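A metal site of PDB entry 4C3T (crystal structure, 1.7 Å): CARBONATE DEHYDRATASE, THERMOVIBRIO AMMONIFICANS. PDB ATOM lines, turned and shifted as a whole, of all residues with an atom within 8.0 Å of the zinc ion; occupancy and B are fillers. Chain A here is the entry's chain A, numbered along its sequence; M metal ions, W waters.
A ring nitrogen (ND1) of His 112 lies within hydrogen-bond range of the side-chain amide oxygen (OE1) of Gln 110 (2.8 Å).
The side-chain carboxylate (OE2) of Glu 129 sits at hydrogen-bond distance from a ring nitrogen (NE2) of His 131 (2.6 Å).
OE1 of Glu 118 sits close to NE2 of His 114, at 3.2 Å.
N of His 114 is in hydrogen-bond range of O of Glu 129 (2.8 Å).
ND1 of His 114 lies within hydrogen-bond range of O of Asn 233.
OE1 of Glu 118 sits at hydrogen-bond distance from OG1 of Thr 198, 2.5 Å away.
The backbone NH (N) of Glu 118 is in hydrogen-bond range of the side-chain carboxylate (OE1) of Glu 129, at 2.8 Å.
Glu 118 touches the zinc ion.
Thr 198 touches the zinc ion.
Of the 22 residues printed, 5 come within 4 Å of the zinc ion.
Along chain A the residues within 4 Å of the zinc ion span positions 112 to 198.
The nearest printed residue that does not touch the zinc ion is Trp 208 (5.4 Å).
The zinc ion is bound by water W1 (2.0 Å), a ring nitrogen (NE2) of His 112 (2.0 Å), a ring nitrogen (ND1) of His 131 (2.1 Å) and a ring nitrogen (NE2) of His 114 (2.1 Å).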
ATOM      1  N   TYR A  28      -9.988 -14.374  -1.426  1.00  0.00           N
ATOM      2  CA  TYR A  28      -9.857 -15.176  -2.635  1.00  0.00           C
ATOM      3  C   TYR A  28     -10.450 -14.546  -3.885  1.00  0.00           C
ATOM      4  O   TYR A  28     -10.376 -15.111  -4.979  1.00  0.00           O
ATOM      5  CB  TYR A  28     -10.418 -16.586  -2.393  1.00  0.00           C
ATOM      6  CG  TYR A  28      -9.496 -17.430  -1.522  1.00  0.00           C
ATOM      7  CD1 TYR A  28      -8.395 -18.086  -2.089  1.00  0.00           C
ATOM      8  CD2 TYR A  28      -9.694 -17.503  -0.151  1.00  0.00           C
ATOM      9  CE1 TYR A  28      -7.538 -18.831  -1.297  1.00  0.00           C
ATOM     10  CE2 TYR A  28      -8.840 -18.253   0.658  1.00  0.00           C
ATOM     11  CZ  TYR A  28      -7.767 -18.905   0.063  1.00  0.00           C
ATOM     12  OH  TYR A  28      -6.924 -19.649   0.841  1.00  0.00           O
ATOM     13  N   HIS A  87     -11.406 -18.175   6.167  1.00  0.00           N
ATOM     14  CA  HIS A  87     -10.580 -18.654   5.062  1.00  0.00           C
ATOM     15  C   HIS A  87     -10.664 -20.173   4.875  1.00  0.00           C
ATOM     16  O   HIS A  87     -10.359 -20.682   3.801  1.00  0.00           O
ATOM     17  CB  HIS A  87      -9.080 -18.317   5.263  1.00  0.00           C
ATOM     18  CG  HIS A  87      -8.784 -16.890   5.623  1.00  0.00           C
ATOM     19  ND1 HIS A  87      -8.946 -15.849   4.734  1.00  0.00           N
ATOM     20  CD2 HIS A  87      -8.284 -16.356   6.753  1.00  0.00           C
ATOM     21  CE1 HIS A  87      -8.573 -14.721   5.318  1.00  0.00           C
ATOM     22  NE2 HIS A  87      -8.164 -15.005   6.543  1.00  0.00           N
ATOM     23  N   THR A  88     -11.024 -20.906   5.939  1.00  0.00           N
ATOM     24  CA  THR A  88     -11.066 -22.366   5.930  1.00  0.00           C
ATOM     25  C   THR A  88     -11.780 -22.831   7.195  1.00  0.00           C
ATOM     26  O   THR A  88     -12.177 -22.007   8.034  1.00  0.00           O
ATOM     27  CB  THR A  88      -9.613 -22.965   5.871  1.00  0.00           C
ATOM     28  OG1 THR A  88      -9.665 -24.370   5.681  1.00  0.00           O
ATOM     29  CG2 THR A  88      -8.874 -22.626   7.189  1.00  0.00           C
ATOM     30  N   GLN A 110      -2.023 -28.278  13.345  1.00  0.00           N
ATOM     31  CA  GLN A 110      -3.401 -27.996  12.880  1.00  0.00           C
ATOM     32  C   GLN A 110      -3.617 -28.698  11.561  1.00  0.00           C
ATOM     33  O   GLN A 110      -2.672 -29.012  10.869  1.00  0.00           O
ATOM     34  CB  GLN A 110      -3.679 -26.488  12.703  1.00  0.00           C
ATOM     35  CG  GLN A 110      -2.650 -25.691  11.905  1.00  0.00           C
ATOM     36  CD  GLN A 110      -3.112 -25.394  10.480  1.00  0.00           C
ATOM     37  OE1 GLN A 110      -3.973 -26.096   9.925  1.00  0.00           O
ATOM     38  NE2 GLN A 110      -2.554 -24.354   9.910  1.00  0.00           N
ATOM     39  N   PHE A 111      -4.873 -28.973  11.227  1.00  0.00           N
ATOM     40  CA  PHE A 111      -5.165 -29.385   9.852  1.00  0.00           C
ATOM     41  C   PHE A 111      -6.395 -28.608   9.362  1.00  0.00           C
ATOM     42  O   PHE A 111      -7.216 -28.174  10.159  1.00  0.00           O
ATOM     43  CB  PHE A 111      -5.285 -30.898   9.659  1.00  0.00           C
ATOM     44  CG  PHE A 111      -6.355 -31.582  10.484  1.00  0.00           C
ATOM     45  CD1 PHE A 111      -7.660 -31.752   9.987  1.00  0.00           C
ATOM     46  CD2 PHE A 111      -6.056 -32.105  11.744  1.00  0.00           C
ATOM     47  CE1 PHE A 111      -8.626 -32.408  10.741  1.00  0.00           C
ATOM     48  CE2 PHE A 111      -7.011 -32.758  12.489  1.00  0.00           C
ATOM     49  CZ  PHE A 111      -8.306 -32.920  11.995  1.00  0.00           C
ATOM     50  N   HIS A 112      -6.467 -28.386   8.050  1.00  0.00           N
ATOM     51  CA  HIS A 112      -7.549 -27.539   7.508  1.00  0.00           C
ATOM     52  C   HIS A 112      -7.801 -27.911   6.071  1.00  0.00           C
ATOM     53  O   HIS A 112      -7.143 -28.765   5.507  1.00  0.00           O
ATOM     54  CB  HIS A 112      -7.177 -26.072   7.602  1.00  0.00           C
ATOM     55  CG  HIS A 112      -6.009 -25.722   6.748  1.00  0.00           C
ATOM     56  ND1 HIS A 112      -4.705 -25.737   7.223  1.00  0.00           N
ATOM     57  CD2 HIS A 112      -5.925 -25.439   5.432  1.00  0.00           C
ATOM     58  CE1 HIS A 112      -3.886 -25.408   6.246  1.00  0.00           C
ATOM     59  NE2 HIS A 112      -4.590 -25.211   5.146  1.00  0.00           N
ATOM     60  N   PHE A 113      -8.781 -27.253   5.446  1.00  0.00           N
ATOM     61  CA  PHE A 113      -9.333 -27.811   4.210  1.00  0.00           C
ATOM     62  C   PHE A 113      -9.519 -26.798   3.086  1.00  0.00           C
ATOM     63  O   PHE A 113      -9.757 -25.625   3.334  1.00  0.00           O
ATOM     64  CB  PHE A 113     -10.688 -28.479   4.528  1.00  0.00           C
ATOM     65  CG  PHE A 113     -10.606 -29.519   5.595  1.00  0.00           C
ATOM     66  CD1 PHE A 113     -10.174 -30.803   5.282  1.00  0.00           C
ATOM     67  CD2 PHE A 113     -10.912 -29.190   6.914  1.00  0.00           C
ATOM     68  CE1 PHE A 113     -10.088 -31.780   6.269  1.00  0.00           C
ATOM     69  CE2 PHE A 113     -10.826 -30.167   7.901  1.00  0.00           C
ATOM     70  CZ  PHE A 113     -10.426 -31.438   7.579  1.00  0.00           C
ATOM     71  N   HIS A 114      -9.440 -27.291   1.842  1.00  0.00           N
ATOM     72  CA  HIS A 114      -9.695 -26.427   0.670  1.00  0.00           C
ATOM     73  C   HIS A 114     -10.624 -27.129  -0.327  1.00  0.00           C
ATOM     74  O   HIS A 114     -10.523 -28.338  -0.542  1.00  0.00           O
ATOM     75  CB  HIS A 114      -8.395 -26.130  -0.053  1.00  0.00           C
ATOM     76  CG  HIS A 114      -7.376 -25.422   0.798  1.00  0.00           C
ATOM     77  ND1 HIS A 114      -7.301 -24.047   0.876  1.00  0.00           N
ATOM     78  CD2 HIS A 114      -6.365 -25.903   1.557  1.00  0.00           C
ATOM     79  CE1 HIS A 114      -6.294 -23.711   1.662  1.00  0.00           C
ATOM     80  NE2 HIS A 114      -5.723 -24.811   2.097  1.00  0.00           N
ATOM     81  N   GLU A 118      -6.042 -27.515  -3.999  1.00  0.00           N
ATOM     82  CA  GLU A 118      -5.072 -26.493  -4.371  1.00  0.00           C
ATOM     83  C   GLU A 118      -4.091 -27.093  -5.363  1.00  0.00           C
ATOM     84  O   GLU A 118      -3.855 -26.533  -6.425  1.00  0.00           O
ATOM     85  CB  GLU A 118      -4.372 -25.969  -3.116  1.00  0.00           C
ATOM     86  CG  GLU A 118      -5.333 -25.345  -2.128  1.00  0.00           C
ATOM     87  CD  GLU A 118      -4.695 -24.221  -1.382  1.00  0.00           C
ATOM     88  OE1 GLU A 118      -3.854 -24.504  -0.513  1.00  0.00           O
ATOM     89  OE2 GLU A 118      -4.995 -23.062  -1.668  1.00  0.00           O
ATOM     90  N   HIS A 119      -3.502 -28.249  -5.023  1.00  0.00           N
ATOM     91  CA  HIS A 119      -2.694 -28.943  -5.997  1.00  0.00           C
ATOM     92  C   HIS A 119      -3.556 -29.568  -7.077  1.00  0.00           C
ATOM     93  O   HIS A 119      -4.693 -29.976  -6.811  1.00  0.00           O
ATOM     94  CB  HIS A 119      -1.815 -29.998  -5.338  1.00  0.00           C
ATOM     95  CG  HIS A 119      -0.740 -29.414  -4.460  1.00  0.00           C
ATOM     96  ND1 HIS A 119      -0.962 -29.092  -3.139  1.00  0.00           N
ATOM     97  CD2 HIS A 119       0.528 -29.064  -4.734  1.00  0.00           C
ATOM     98  CE1 HIS A 119       0.139 -28.566  -2.633  1.00  0.00           C
ATOM     99  NE2 HIS A 119       1.063 -28.549  -3.572  1.00  0.00           N
ATOM    100  N   GLU A 129      -9.194 -30.878  -0.678  1.00  0.00           N
ATOM    101  CA  GLU A 129      -7.813 -31.192  -0.263  1.00  0.00           C
ATOM    102  C   GLU A 129      -7.638 -30.783   1.200  1.00  0.00           C
ATOM    103  O   GLU A 129      -8.035 -29.692   1.580  1.00  0.00           O
ATOM    104  CB  GLU A 129      -6.813 -30.468  -1.169  1.00  0.00           C
ATOM    105  CG  GLU A 129      -5.318 -30.725  -0.858  1.00  0.00           C
ATOM    106  CD  GLU A 129      -4.356 -30.036  -1.817  1.00  0.00           C
ATOM    107  OE1 GLU A 129      -4.736 -29.764  -2.972  1.00  0.00           O
ATOM    108  OE2 GLU A 129      -3.180 -29.777  -1.448  1.00  0.00           O
ATOM    109  N   ALA A 130      -7.053 -31.677   2.014  1.00  0.00           N
ATOM    110  CA  ALA A 130      -6.749 -31.411   3.429  1.00  0.00           C
ATOM    111  C   ALA A 130      -5.247 -31.191   3.570  1.00  0.00           C
ATOM    112  O   ALA A 130      -4.457 -31.823   2.862  1.00  0.00           O
ATOM    113  CB  ALA A 130      -7.159 -32.597   4.286  1.00  0.00           C
ATOM    114  N   HIS A 131      -4.882 -30.238   4.435  1.00  0.00           N
ATOM    115  CA  HIS A 131      -3.474 -29.920   4.710  1.00  0.00           C
ATOM    116  C   HIS A 131      -3.248 -30.162   6.177  1.00  0.00           C
ATOM    117  O   HIS A 131      -3.978 -29.632   7.010  1.00  0.00           O
ATOM    118  CB  HIS A 131      -3.228 -28.459   4.363  1.00  0.00           C
ATOM    119  CG  HIS A 131      -3.184 -28.212   2.898  1.00  0.00           C
ATOM    120  ND1 HIS A 131      -3.318 -26.958   2.333  1.00  0.00           N
ATOM    121  CD2 HIS A 131      -2.995 -29.080   1.877  1.00  0.00           C
ATOM    122  CE1 HIS A 131      -3.233 -27.077   1.020  1.00  0.00           C
ATOM    123  NE2 HIS A 131      -3.054 -28.346   0.719  1.00  0.00           N
ATOM    124  N   PHE A 132      -2.208 -30.950   6.473  1.00  0.00           N
ATOM    125  CA  PHE A 132      -1.826 -31.204   7.869  1.00  0.00           C
ATOM    126  C   PHE A 132      -0.509 -30.449   8.079  1.00  0.00           C
ATOM    127  O   PHE A 132       0.473 -30.764   7.406  1.00  0.00           O
ATOM    128  CB  PHE A 132      -1.677 -32.699   8.062  1.00  0.00           C
ATOM    129  CG  PHE A 132      -2.946 -33.478   7.885  1.00  0.00           C
ATOM    130  CD1 PHE A 132      -3.394 -33.846   6.600  1.00  0.00           C
ATOM    131  CD2 PHE A 132      -3.712 -33.845   8.989  1.00  0.00           C
ATOM    132  CE1 PHE A 132      -4.566 -34.571   6.448  1.00  0.00           C
ATOM    133  CE2 PHE A 132      -4.899 -34.554   8.826  1.00  0.00           C
ATOM    134  CZ  PHE A 132      -5.313 -34.914   7.550  1.00  0.00           C
ATOM    135  N   VAL A 133      -0.517 -29.451   8.966  1.00  0.00           N
ATOM    136  CA  VAL A 133       0.577 -28.487   9.085  1.00  0.00           C
ATOM    137  C   VAL A 133       1.427 -28.852  10.314  1.00  0.00           C
ATOM    138  O   VAL A 133       0.888 -28.948  11.413  1.00  0.00           O
ATOM    139  CB  VAL A 133       0.047 -27.054   9.217  1.00  0.00           C
ATOM    140  CG1 VAL A 133       1.175 -26.044   9.281  1.00  0.00           C
ATOM    141  CG2 VAL A 133      -0.834 -26.684   8.019  1.00  0.00           C
ATOM    142  N   VAL A 143       4.119 -29.750   5.350  1.00  0.00           N
ATOM    143  CA  VAL A 143       2.695 -29.899   5.156  1.00  0.00           C
ATOM    144  C   VAL A 143       2.439 -31.223   4.430  1.00  0.00           C
ATOM    145  O   VAL A 143       3.080 -31.507   3.407  1.00  0.00           O
ATOM    146  CB  VAL A 143       2.078 -28.712   4.354  1.00  0.00           C
ATOM    147  CG1 VAL A 143       0.548 -28.870   4.405  1.00  0.00           C
ATOM    148  CG2 VAL A 143       2.444 -27.371   4.959  1.00  0.00           C
ATOM    149  N   LEU A 144       1.537 -32.051   4.972  1.00  0.00           N
ATOM    150  CA  LEU A 144       1.080 -33.249   4.307  1.00  0.00           C
ATOM    151  C   LEU A 144      -0.253 -32.914   3.634  1.00  0.00           C
ATOM    152  O   LEU A 144      -1.117 -32.330   4.268  1.00  0.00           O
ATOM    153  CB  LEU A 144       0.865 -34.407   5.285  1.00  0.00           C
ATOM    154  CG  LEU A 144       2.053 -35.323   5.473  1.00  0.00           C
ATOM    155  CD1 LEU A 144       3.291 -34.513   5.882  1.00  0.00           C
ATOM    156  CD2 LEU A 144       1.696 -36.376   6.506  1.00  0.00           C
ATOM    157  N   LEU A 197       3.955 -21.842   1.963  1.00  0.00           N
ATOM    158  CA  LEU A 197       2.578 -21.821   2.479  1.00  0.00           C
ATOM    159  C   LEU A 197       1.708 -21.309   1.330  1.00  0.00           C
ATOM    160  O   LEU A 197       2.152 -20.501   0.518  1.00  0.00           O
ATOM    161  CB  LEU A 197       2.428 -20.913   3.692  1.00  0.00           C
ATOM    162  CG  LEU A 197       3.289 -21.240   4.916  1.00  0.00           C
ATOM    163  CD1 LEU A 197       3.038 -20.155   5.955  1.00  0.00           C
ATOM    164  CD2 LEU A 197       2.939 -22.601   5.450  1.00  0.00           C
ATOM    165  N   THR A 198       0.464 -21.780   1.282  1.00  0.00           N
ATOM    166  CA  THR A 198      -0.446 -21.374   0.202  1.00  0.00           C
ATOM    167  C   THR A 198      -1.344 -20.227   0.590  1.00  0.00           C
ATOM    168  O   THR A 198      -2.214 -19.831  -0.207  1.00  0.00           O
ATOM    169  CB  THR A 198      -1.330 -22.552  -0.293  1.00  0.00           C
ATOM    170  OG1 THR A 198      -2.282 -22.926   0.697  1.00  0.00           O
ATOM    171  CG2 THR A 198      -0.491 -23.773  -0.704  1.00  0.00           C
ATOM    172  N   THR A 199      -1.154 -19.688   1.786  1.00  0.00           N
ATOM    173  CA  THR A 199      -1.885 -18.513   2.253  1.00  0.00           C
ATOM    174  C   THR A 199      -0.854 -17.513   2.792  1.00  0.00           C
ATOM    175  O   THR A 199       0.253 -17.940   3.195  1.00  0.00           O
ATOM    176  CB  THR A 199      -2.931 -18.844   3.327  1.00  0.00           C
ATOM    177  OG1 THR A 199      -2.308 -19.527   4.443  1.00  0.00           O
ATOM    178  CG2 THR A 199      -4.014 -19.792   2.762  1.00  0.00           C
ATOM    179  N   TRP A 208       6.781 -30.130   1.161  1.00  0.00           N
ATOM    180  CA  TRP A 208       5.470 -30.650   0.792  1.00  0.00           C
ATOM    181  C   TRP A 208       5.520 -32.159   0.559  1.00  0.00           C
ATOM    182  O   TRP A 208       6.366 -32.682  -0.190  1.00  0.00           O
ATOM    183  CB  TRP A 208       4.899 -29.907  -0.438  1.00  0.00           C
ATOM    184  CG  TRP A 208       4.244 -28.638  -0.090  1.00  0.00           C
ATOM    185  CD1 TRP A 208       4.801 -27.385  -0.095  1.00  0.00           C
ATOM    186  CD2 TRP A 208       2.902 -28.478   0.339  1.00  0.00           C
ATOM    187  NE1 TRP A 208       3.877 -26.451   0.320  1.00  0.00           N
ATOM    188  CE2 TRP A 208       2.691 -27.087   0.574  1.00  0.00           C
ATOM    189  CE3 TRP A 208       1.840 -29.370   0.522  1.00  0.00           C
ATOM    190  CZ2 TRP A 208       1.462 -26.581   1.008  1.00  0.00           C
ATOM    191  CZ3 TRP A 208       0.608 -28.855   0.946  1.00  0.00           C
ATOM    192  CH2 TRP A 208       0.440 -27.474   1.180  1.00  0.00           C
ATOM    193  N   ASN A 233     -11.800 -21.676  -2.007  1.00  0.00           N
ATOM    194  CA  ASN A 233     -10.705 -21.154  -1.170  1.00  0.00           C
ATOM    195  C   ASN A 233      -9.347 -21.776  -1.549  1.00  0.00           C
ATOM    196  O   ASN A 233      -8.516 -22.063  -0.671  1.00  0.00           O
ATOM    197  CB  ASN A 233     -11.015 -21.311   0.329  1.00  0.00           C
ATOM    198  CG  ASN A 233     -10.987 -22.763   0.789  1.00  0.00           C
ATOM    199  OD1 ASN A 233     -11.177 -23.685  -0.006  1.00  0.00           O
ATOM    200  ND2 ASN A 233     -10.754 -22.980   2.083  1.00  0.00           N
HETATM  201 ZN    ZN M   1      -4.016 -25.214   3.195  1.00  0.00          ZN
HETATM  202  O   HOH W   1      -2.714 -23.754   3.089  1.00  0.00           O
